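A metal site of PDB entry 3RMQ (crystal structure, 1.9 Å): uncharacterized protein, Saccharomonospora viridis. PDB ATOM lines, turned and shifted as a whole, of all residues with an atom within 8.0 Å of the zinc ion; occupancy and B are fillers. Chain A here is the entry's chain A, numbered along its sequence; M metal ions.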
ATOM      1  N   TRP A   9     -28.487 -17.941  34.832  1.00  0.00           N
ATOM      2  CA  TRP A   9     -27.359 -18.017  33.919  1.00  0.00           C
ATOM      3  C   TRP A   9     -26.304 -18.962  34.472  1.00  0.00           C
ATOM      4  O   TRP A   9     -26.134 -19.044  35.715  1.00  0.00           O
ATOM      5  CB  TRP A   9     -26.762 -16.595  33.713  1.00  0.00           C
ATOM      6  CG  TRP A   9     -27.716 -15.689  32.999  1.00  0.00           C
ATOM      7  CD1 TRP A   9     -28.742 -14.935  33.565  1.00  0.00           C
ATOM      8  CD2 TRP A   9     -27.765 -15.447  31.578  1.00  0.00           C
ATOM      9  NE1 TRP A   9     -29.414 -14.252  32.550  1.00  0.00           N
ATOM     10  CE2 TRP A   9     -28.827 -14.527  31.340  1.00  0.00           C
ATOM     11  CE3 TRP A   9     -27.014 -15.911  30.480  1.00  0.00           C
ATOM     12  CZ2 TRP A   9     -29.176 -14.080  30.036  1.00  0.00           C
ATOM     13  CZ3 TRP A   9     -27.354 -15.446  29.162  1.00  0.00           C
ATOM     14  CH2 TRP A   9     -28.417 -14.549  28.978  1.00  0.00           C
ATOM     15  N   GLN A  10     -25.560 -19.613  33.570  1.00  0.00           N
ATOM     16  CA  GLN A  10     -24.399 -20.404  33.970  1.00  0.00           C
ATOM     17  C   GLN A  10     -23.415 -20.494  32.820  1.00  0.00           C
ATOM     18  O   GLN A  10     -23.800 -20.882  31.706  1.00  0.00           O
ATOM     19  CB  GLN A  10     -24.847 -21.829  34.389  1.00  0.00           C
ATOM     20  CG  GLN A  10     -23.675 -22.811  34.637  1.00  0.00           C
ATOM     21  CD  GLN A  10     -22.784 -22.359  35.784  1.00  0.00           C
ATOM     22  OE1 GLN A  10     -23.278 -22.086  36.873  1.00  0.00           O
ATOM     23  NE2 GLN A  10     -21.461 -22.234  35.528  1.00  0.00           N
ATOM     24  N   ALA A  12     -20.591 -22.106  30.607  1.00  0.00           N
ATOM     25  CA  ALA A  12     -20.090 -23.456  30.343  1.00  0.00           C
ATOM     26  C   ALA A  12     -19.806 -23.607  28.871  1.00  0.00           C
ATOM     27  O   ALA A  12     -20.505 -23.052  28.029  1.00  0.00           O
ATOM     28  CB  ALA A  12     -21.143 -24.517  30.780  1.00  0.00           C
ATOM     29  N   LYS A  15     -19.640 -20.282  26.591  1.00  0.00           N
ATOM     30  CA  LYS A  15     -20.644 -19.219  26.539  1.00  0.00           C
ATOM     31  C   LYS A  15     -21.361 -19.114  27.849  1.00  0.00           C
ATOM     32  O   LYS A  15     -21.358 -20.049  28.641  1.00  0.00           O
ATOM     33  CB  LYS A  15     -21.714 -19.521  25.478  1.00  0.00           C
ATOM     34  CG  LYS A  15     -21.187 -19.922  24.059  1.00  0.00           C
ATOM     35  CD  LYS A  15     -22.387 -20.297  23.165  1.00  0.00           C
ATOM     36  CE  LYS A  15     -21.989 -20.945  21.830  1.00  0.00           C
ATOM     37  NZ  LYS A  15     -22.044 -22.442  21.918  1.00  0.00           N
ATOM     38  N   ARG A  16     -22.066 -18.011  28.052  1.00  0.00           N
ATOM     39  CA  ARG A  16     -22.893 -17.904  29.233  1.00  0.00           C
ATOM     40  C   ARG A  16     -24.312 -18.360  28.845  1.00  0.00           C
ATOM     41  O   ARG A  16     -24.991 -17.671  28.079  1.00  0.00           O
ATOM     42  CB  ARG A  16     -22.904 -16.455  29.766  1.00  0.00           C
ATOM     43  CG  ARG A  16     -23.330 -16.459  31.225  1.00  0.00           C
ATOM     44  CD  ARG A  16     -23.524 -15.064  31.811  1.00  0.00           C
ATOM     45  NE  ARG A  16     -22.245 -14.351  31.876  1.00  0.00           N
ATOM     46  CZ  ARG A  16     -22.067 -13.141  32.443  1.00  0.00           C
ATOM     47  NH1 ARG A  16     -23.107 -12.490  32.966  1.00  0.00           N
ATOM     48  NH2 ARG A  16     -20.836 -12.600  32.479  1.00  0.00           N
ATOM     49  N   HIS A  17     -24.699 -19.579  29.273  1.00  0.00           N
ATOM     50  CA  HIS A  17     -25.978 -20.155  28.863  1.00  0.00           C
ATOM     51  C   HIS A  17     -27.017 -19.854  29.914  1.00  0.00           C
ATOM     52  O   HIS A  17     -26.670 -19.291  30.982  1.00  0.00           O
ATOM     53  CB  HIS A  17     -25.873 -21.685  28.697  1.00  0.00           C
ATOM     54  CG  HIS A  17     -24.982 -22.111  27.574  1.00  0.00           C
ATOM     55  ND1 HIS A  17     -25.399 -22.149  26.260  1.00  0.00           N
ATOM     56  CD2 HIS A  17     -23.687 -22.514  27.575  1.00  0.00           C
ATOM     57  CE1 HIS A  17     -24.412 -22.612  25.502  1.00  0.00           C
ATOM     58  NE2 HIS A  17     -23.350 -22.815  26.285  1.00  0.00           N
ATOM     59  N   VAL A  18     -28.271 -20.225  29.636  1.00  0.00           N
ATOM     60  CA  VAL A  18     -29.378 -20.045  30.583  1.00  0.00           C
ATOM     61  C   VAL A  18     -29.865 -21.447  30.826  1.00  0.00           C
ATOM     62  O   VAL A  18     -29.876 -22.291  29.876  1.00  0.00           O
ATOM     63  CB  VAL A  18     -30.530 -19.190  29.998  1.00  0.00           C
ATOM     64  CG1 VAL A  18     -31.719 -19.175  30.943  1.00  0.00           C
ATOM     65  CG2 VAL A  18     -30.028 -17.753  29.772  1.00  0.00           C
ATOM     66  N   TYR A  19     -30.237 -21.744  32.066  1.00  0.00           N
ATOM     67  CA  TYR A  19     -30.869 -23.044  32.299  1.00  0.00           C
ATOM     68  C   TYR A  19     -32.183 -22.895  33.086  1.00  0.00           C
ATOM     69  O   TYR A  19     -32.427 -21.884  33.765  1.00  0.00           O
ATOM     70  CB  TYR A  19     -29.890 -24.013  33.015  1.00  0.00           C
ATOM     71  CG  TYR A  19     -29.580 -23.677  34.433  1.00  0.00           C
ATOM     72  CD1 TYR A  19     -28.654 -22.683  34.754  1.00  0.00           C
ATOM     73  CD2 TYR A  19     -30.214 -24.343  35.479  1.00  0.00           C
ATOM     74  CE1 TYR A  19     -28.389 -22.344  36.071  1.00  0.00           C
ATOM     75  CE2 TYR A  19     -29.948 -24.012  36.807  1.00  0.00           C
ATOM     76  CZ  TYR A  19     -29.036 -23.015  37.096  1.00  0.00           C
ATOM     77  OH  TYR A  19     -28.775 -22.697  38.407  1.00  0.00           O
ATOM     78  N   PHE A  32     -25.385 -30.210  32.233  1.00  0.00           N
ATOM     79  CA  PHE A  32     -26.776 -29.796  32.198  1.00  0.00           C
ATOM     80  C   PHE A  32     -27.112 -29.410  30.782  1.00  0.00           C
ATOM     81  O   PHE A  32     -26.222 -29.213  29.968  1.00  0.00           O
ATOM     82  CB  PHE A  32     -27.027 -28.635  33.168  1.00  0.00           C
ATOM     83  CG  PHE A  32     -26.360 -27.313  32.758  1.00  0.00           C
ATOM     84  CD1 PHE A  32     -25.034 -27.048  33.108  1.00  0.00           C
ATOM     85  CD2 PHE A  32     -27.058 -26.353  32.036  1.00  0.00           C
ATOM     86  CE1 PHE A  32     -24.413 -25.828  32.732  1.00  0.00           C
ATOM     87  CE2 PHE A  32     -26.449 -25.139  31.639  1.00  0.00           C
ATOM     88  CZ  PHE A  32     -25.111 -24.873  31.997  1.00  0.00           C
ATOM     89  N   THR A  33     -28.390 -29.312  30.477  1.00  0.00           N
ATOM     90  CA  THR A  33     -28.782 -28.915  29.148  1.00  0.00           C
ATOM     91  C   THR A  33     -29.375 -27.523  29.267  1.00  0.00           C
ATOM     92  O   THR A  33     -30.293 -27.267  30.061  1.00  0.00           O
ATOM     93  CB  THR A  33     -29.840 -29.867  28.560  1.00  0.00           C
ATOM     94  OG1 THR A  33     -29.259 -31.185  28.474  1.00  0.00           O
ATOM     95  CG2 THR A  33     -30.240 -29.413  27.178  1.00  0.00           C
ATOM     96  N   ALA A  34     -28.822 -26.616  28.482  1.00  0.00           N
ATOM     97  CA  ALA A  34     -29.253 -25.220  28.476  1.00  0.00           C
ATOM     98  C   ALA A  34     -30.564 -25.016  27.679  1.00  0.00           C
ATOM     99  O   ALA A  34     -31.037 -25.913  26.944  1.00  0.00           O
ATOM    100  CB  ALA A  34     -28.161 -24.395  27.858  1.00  0.00           C
ATOM    101  N   LEU A  35     -31.140 -23.816  27.744  1.00  0.00           N
ATOM    102  CA  LEU A  35     -32.382 -23.552  26.969  1.00  0.00           C
ATOM    103  C   LEU A  35     -32.130 -23.744  25.468  1.00  0.00           C
ATOM    104  O   LEU A  35     -33.032 -24.073  24.699  1.00  0.00           O
ATOM    105  CB  LEU A  35     -32.888 -22.115  27.175  1.00  0.00           C
ATOM    106  CG  LEU A  35     -33.369 -21.731  28.547  1.00  0.00           C
ATOM    107  CD1 LEU A  35     -34.020 -20.321  28.453  1.00  0.00           C
ATOM    108  CD2 LEU A  35     -34.297 -22.812  29.106  1.00  0.00           C
ATOM    109  N   CYS A  36     -30.889 -23.565  25.039  1.00  0.00           N
ATOM    110  CA  CYS A  36     -30.609 -23.663  23.599  1.00  0.00           C
ATOM    111  C   CYS A  36     -30.491 -25.101  23.160  1.00  0.00           C
ATOM    112  O   CYS A  36     -30.337 -25.403  21.947  1.00  0.00           O
ATOM    113  CB  CYS A  36     -29.287 -22.928  23.252  1.00  0.00           C
ATOM    114  SG  CYS A  36     -27.849 -23.633  24.073  1.00  0.00           S
ATOM    115  N   GLY A  37     -30.523 -26.016  24.126  1.00  0.00           N
ATOM    116  CA  GLY A  37     -30.462 -27.430  23.777  1.00  0.00           C
ATOM    117  C   GLY A  37     -29.092 -28.080  23.845  1.00  0.00           C
ATOM    118  O   GLY A  37     -28.986 -29.287  23.770  1.00  0.00           O
ATOM    119  N   GLU A  38     -28.043 -27.289  24.010  1.00  0.00           N
ATOM    120  CA  GLU A  38     -26.686 -27.831  24.165  1.00  0.00           C
ATOM    121  C   GLU A  38     -26.498 -28.423  25.565  1.00  0.00           C
ATOM    122  O   GLU A  38     -26.842 -27.784  26.561  1.00  0.00           O
ATOM    123  CB  GLU A  38     -25.639 -26.737  23.936  1.00  0.00           C
ATOM    124  CG  GLU A  38     -25.520 -26.275  22.486  1.00  0.00           C
ATOM    125  CD  GLU A  38     -24.915 -27.333  21.580  1.00  0.00           C
ATOM    126  OE1 GLU A  38     -23.680 -27.519  21.624  1.00  0.00           O
ATOM    127  OE2 GLU A  38     -25.663 -27.981  20.831  1.00  0.00           O
ATOM    128  N   VAL A  40     -23.943 -29.234  28.340  1.00  0.00           N
ATOM    129  CA  VAL A  40     -22.621 -28.665  28.630  1.00  0.00           C
ATOM    130  C   VAL A  40     -22.257 -28.963  30.095  1.00  0.00           C
ATOM    131  O   VAL A  40     -23.147 -29.222  30.896  1.00  0.00           O
ATOM    132  CB  VAL A  40     -22.600 -27.123  28.411  1.00  0.00           C
ATOM    133  CG1 VAL A  40     -22.723 -26.784  26.868  1.00  0.00           C
ATOM    134  CG2 VAL A  40     -23.730 -26.492  29.209  1.00  0.00           C
ATOM    135  N   GLU A  58     -22.317 -14.036  26.208  1.00  0.00           N
ATOM    136  CA  GLU A  58     -23.606 -14.717  26.359  1.00  0.00           C
ATOM    137  C   GLU A  58     -23.945 -15.603  25.146  1.00  0.00           C
ATOM    138  O   GLU A  58     -23.643 -15.262  24.003  1.00  0.00           O
ATOM    139  CB  GLU A  58     -24.726 -13.704  26.570  1.00  0.00           C
ATOM    140  CG  GLU A  58     -24.716 -13.110  27.947  1.00  0.00           C
ATOM    141  CD  GLU A  58     -23.687 -12.000  28.130  1.00  0.00           C
ATOM    142  OE1 GLU A  58     -23.411 -11.262  27.148  1.00  0.00           O
ATOM    143  OE2 GLU A  58     -23.134 -11.888  29.269  1.00  0.00           O
ATOM    144  N   CYS A  59     -24.594 -16.726  25.393  1.00  0.00           N
ATOM    145  CA  CYS A  59     -25.099 -17.617  24.350  1.00  0.00           C
ATOM    146  C   CYS A  59     -26.249 -16.895  23.643  1.00  0.00           C
ATOM    147  O   CYS A  59     -27.248 -16.550  24.273  1.00  0.00           O
ATOM    148  CB  CYS A  59     -25.629 -18.937  24.979  1.00  0.00           C
ATOM    149  SG  CYS A  59     -26.458 -19.997  23.709  1.00  0.00           S
ATOM    150  N   PRO A  60     -26.103 -16.580  22.336  1.00  0.00           N
ATOM    151  CA  PRO A  60     -27.201 -15.826  21.692  1.00  0.00           C
ATOM    152  C   PRO A  60     -28.505 -16.598  21.718  1.00  0.00           C
ATOM    153  O   PRO A  60     -29.581 -16.002  21.860  1.00  0.00           O
ATOM    154  CB  PRO A  60     -26.714 -15.679  20.229  1.00  0.00           C
ATOM    155  CG  PRO A  60     -25.194 -15.720  20.351  1.00  0.00           C
ATOM    156  CD  PRO A  60     -24.946 -16.763  21.443  1.00  0.00           C
ATOM    157  N   VAL A  61     -28.444 -17.925  21.555  1.00  0.00           N
ATOM    158  CA  VAL A  61     -29.688 -18.697  21.474  1.00  0.00           C
ATOM    159  C   VAL A  61     -30.426 -18.713  22.818  1.00  0.00           C
ATOM    160  O   VAL A  61     -31.639 -18.458  22.898  1.00  0.00           O
ATOM    161  CB  VAL A  61     -29.373 -20.137  21.027  1.00  0.00           C
ATOM    162  CG1 VAL A  61     -30.619 -20.968  21.054  1.00  0.00           C
ATOM    163  CG2 VAL A  61     -28.760 -20.081  19.577  1.00  0.00           C
ATOM    164  N   CYS A  62     -29.687 -18.996  23.886  1.00  0.00           N
ATOM    165  CA  CYS A  62     -30.262 -18.955  25.236  1.00  0.00           C
ATOM    166  C   CYS A  62     -30.849 -17.574  25.571  1.00  0.00           C
ATOM    167  O   CYS A  62     -31.891 -17.488  26.228  1.00  0.00           O
ATOM    168  CB  CYS A  62     -29.192 -19.285  26.297  1.00  0.00           C
ATOM    169  SG  CYS A  62     -28.892 -21.026  26.511  1.00  0.00           S
ATOM    170  N   THR A  63     -30.167 -16.504  25.178  1.00  0.00           N
ATOM    171  CA  THR A  63     -30.625 -15.140  25.520  1.00  0.00           C
ATOM    172  C   THR A  63     -31.995 -14.863  24.869  1.00  0.00           C
ATOM    173  O   THR A  63     -32.911 -14.362  25.512  1.00  0.00           O
ATOM    174  CB  THR A  63     -29.600 -14.049  25.047  1.00  0.00           C
ATOM    175  OG1 THR A  63     -28.302 -14.268  25.652  1.00  0.00           O
ATOM    176  CG2 THR A  63     -30.088 -12.600  25.424  1.00  0.00           C
ATOM    177  N   ALA A  65     -34.051 -17.245  23.609  1.00  0.00           N
ATOM    178  CA  ALA A  65     -35.007 -18.236  24.170  1.00  0.00           C
ATOM    179  C   ALA A  65     -35.586 -17.742  25.515  1.00  0.00           C
ATOM    180  O   ALA A  65     -36.791 -17.847  25.754  1.00  0.00           O
ATOM    181  CB  ALA A  65     -34.378 -19.571  24.326  1.00  0.00           C
ATOM    182  N   LEU A  90     -25.763 -21.354  15.035  1.00  0.00           N
ATOM    183  CA  LEU A  90     -26.618 -20.708  16.046  1.00  0.00           C
ATOM    184  C   LEU A  90     -28.021 -20.443  15.553  1.00  0.00           C
ATOM    185  O   LEU A  90     -28.966 -20.639  16.284  1.00  0.00           O
ATOM    186  CB  LEU A  90     -26.027 -19.378  16.501  1.00  0.00           C
ATOM    187  CG  LEU A  90     -24.742 -19.606  17.300  1.00  0.00           C
ATOM    188  CD1 LEU A  90     -23.975 -18.328  17.448  1.00  0.00           C
ATOM    189  CD2 LEU A  90     -25.160 -20.141  18.666  1.00  0.00           C
ATOM    190  N   ARG A  93     -29.915 -23.610  15.336  1.00  0.00           N
ATOM    191  CA  ARG A  93     -30.217 -24.020  16.704  1.00  0.00           C
ATOM    192  C   ARG A  93     -31.394 -23.184  17.299  1.00  0.00           C
ATOM    193  O   ARG A  93     -32.285 -23.736  17.944  1.00  0.00           O
ATOM    194  CB  ARG A  93     -28.952 -23.894  17.575  1.00  0.00           C
ATOM    195  CG  ARG A  93     -29.127 -24.388  19.007  1.00  0.00           C
ATOM    196  CD  ARG A  93     -27.730 -24.364  19.773  1.00  0.00           C
ATOM    197  NE  ARG A  93     -26.740 -25.179  19.064  1.00  0.00           N
ATOM    198  CZ  ARG A  93     -25.458 -24.842  18.861  1.00  0.00           C
ATOM    199  NH1 ARG A  93     -24.978 -23.693  19.306  1.00  0.00           N
ATOM    200  NH2 ARG A  93     -24.640 -25.664  18.187  1.00  0.00           N
HETATM  201 ZN    ZN M   1     -27.133 -21.668  25.218  1.00  0.00          ZN
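The backbone carbonyl oxygen (O) of Ala 12 sits close to a ring nitrogen (NE2) of His 17, at 3.3 Å. The backbone carbonyl oxygen (O) of His 17 lies within hydrogen-bond range of the backbone NH (N) of Gln 10 (2.8 Å). The side-chain sulfur (SG) of Cys 62 sits close to the backbone NH (N) of Val 18 (3.3 Å). The side-chain sulfur (SG) of Cys 62 lies close to the backbone NH (N) of Leu 35 (3.8 Å). The side-chain sulfur (SG) of Cys 59 sits close to the backbone NH (N) of Val 61, 3.6 Å away. The backbone NH of Cys 59 sits at hydrogen-bond distance from the backbone carbonyl oxygen of Arg 16. O of Cys 59 lies within hydrogen-bond range of OG1 of Thr 63, at 2.9 Å. The side-chain sulfur of Cys 36 lies close to the backbone NH of Glu 38, 3.7 Å away.
Merely in contact with the zinc ion: Ala 34. Within 4 Å of the zinc ion: His 17, Ala 34, Cys 36, Cys 59 and Cys 62. The nearest printed residue that does not touch the zinc ion is Val 18 (4.8 Å).
The zinc ion is bound by a ring nitrogen (ND1) of His 17 (2.1 Å), the side-chain sulfur of Cys 62 (2.3 Å), the side-chain sulfur of Cys 59 (2.4 Å) and the side-chain sulfur of Cys 36 (2.4 Å). The zinc ion has four donor atoms within binding distance.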
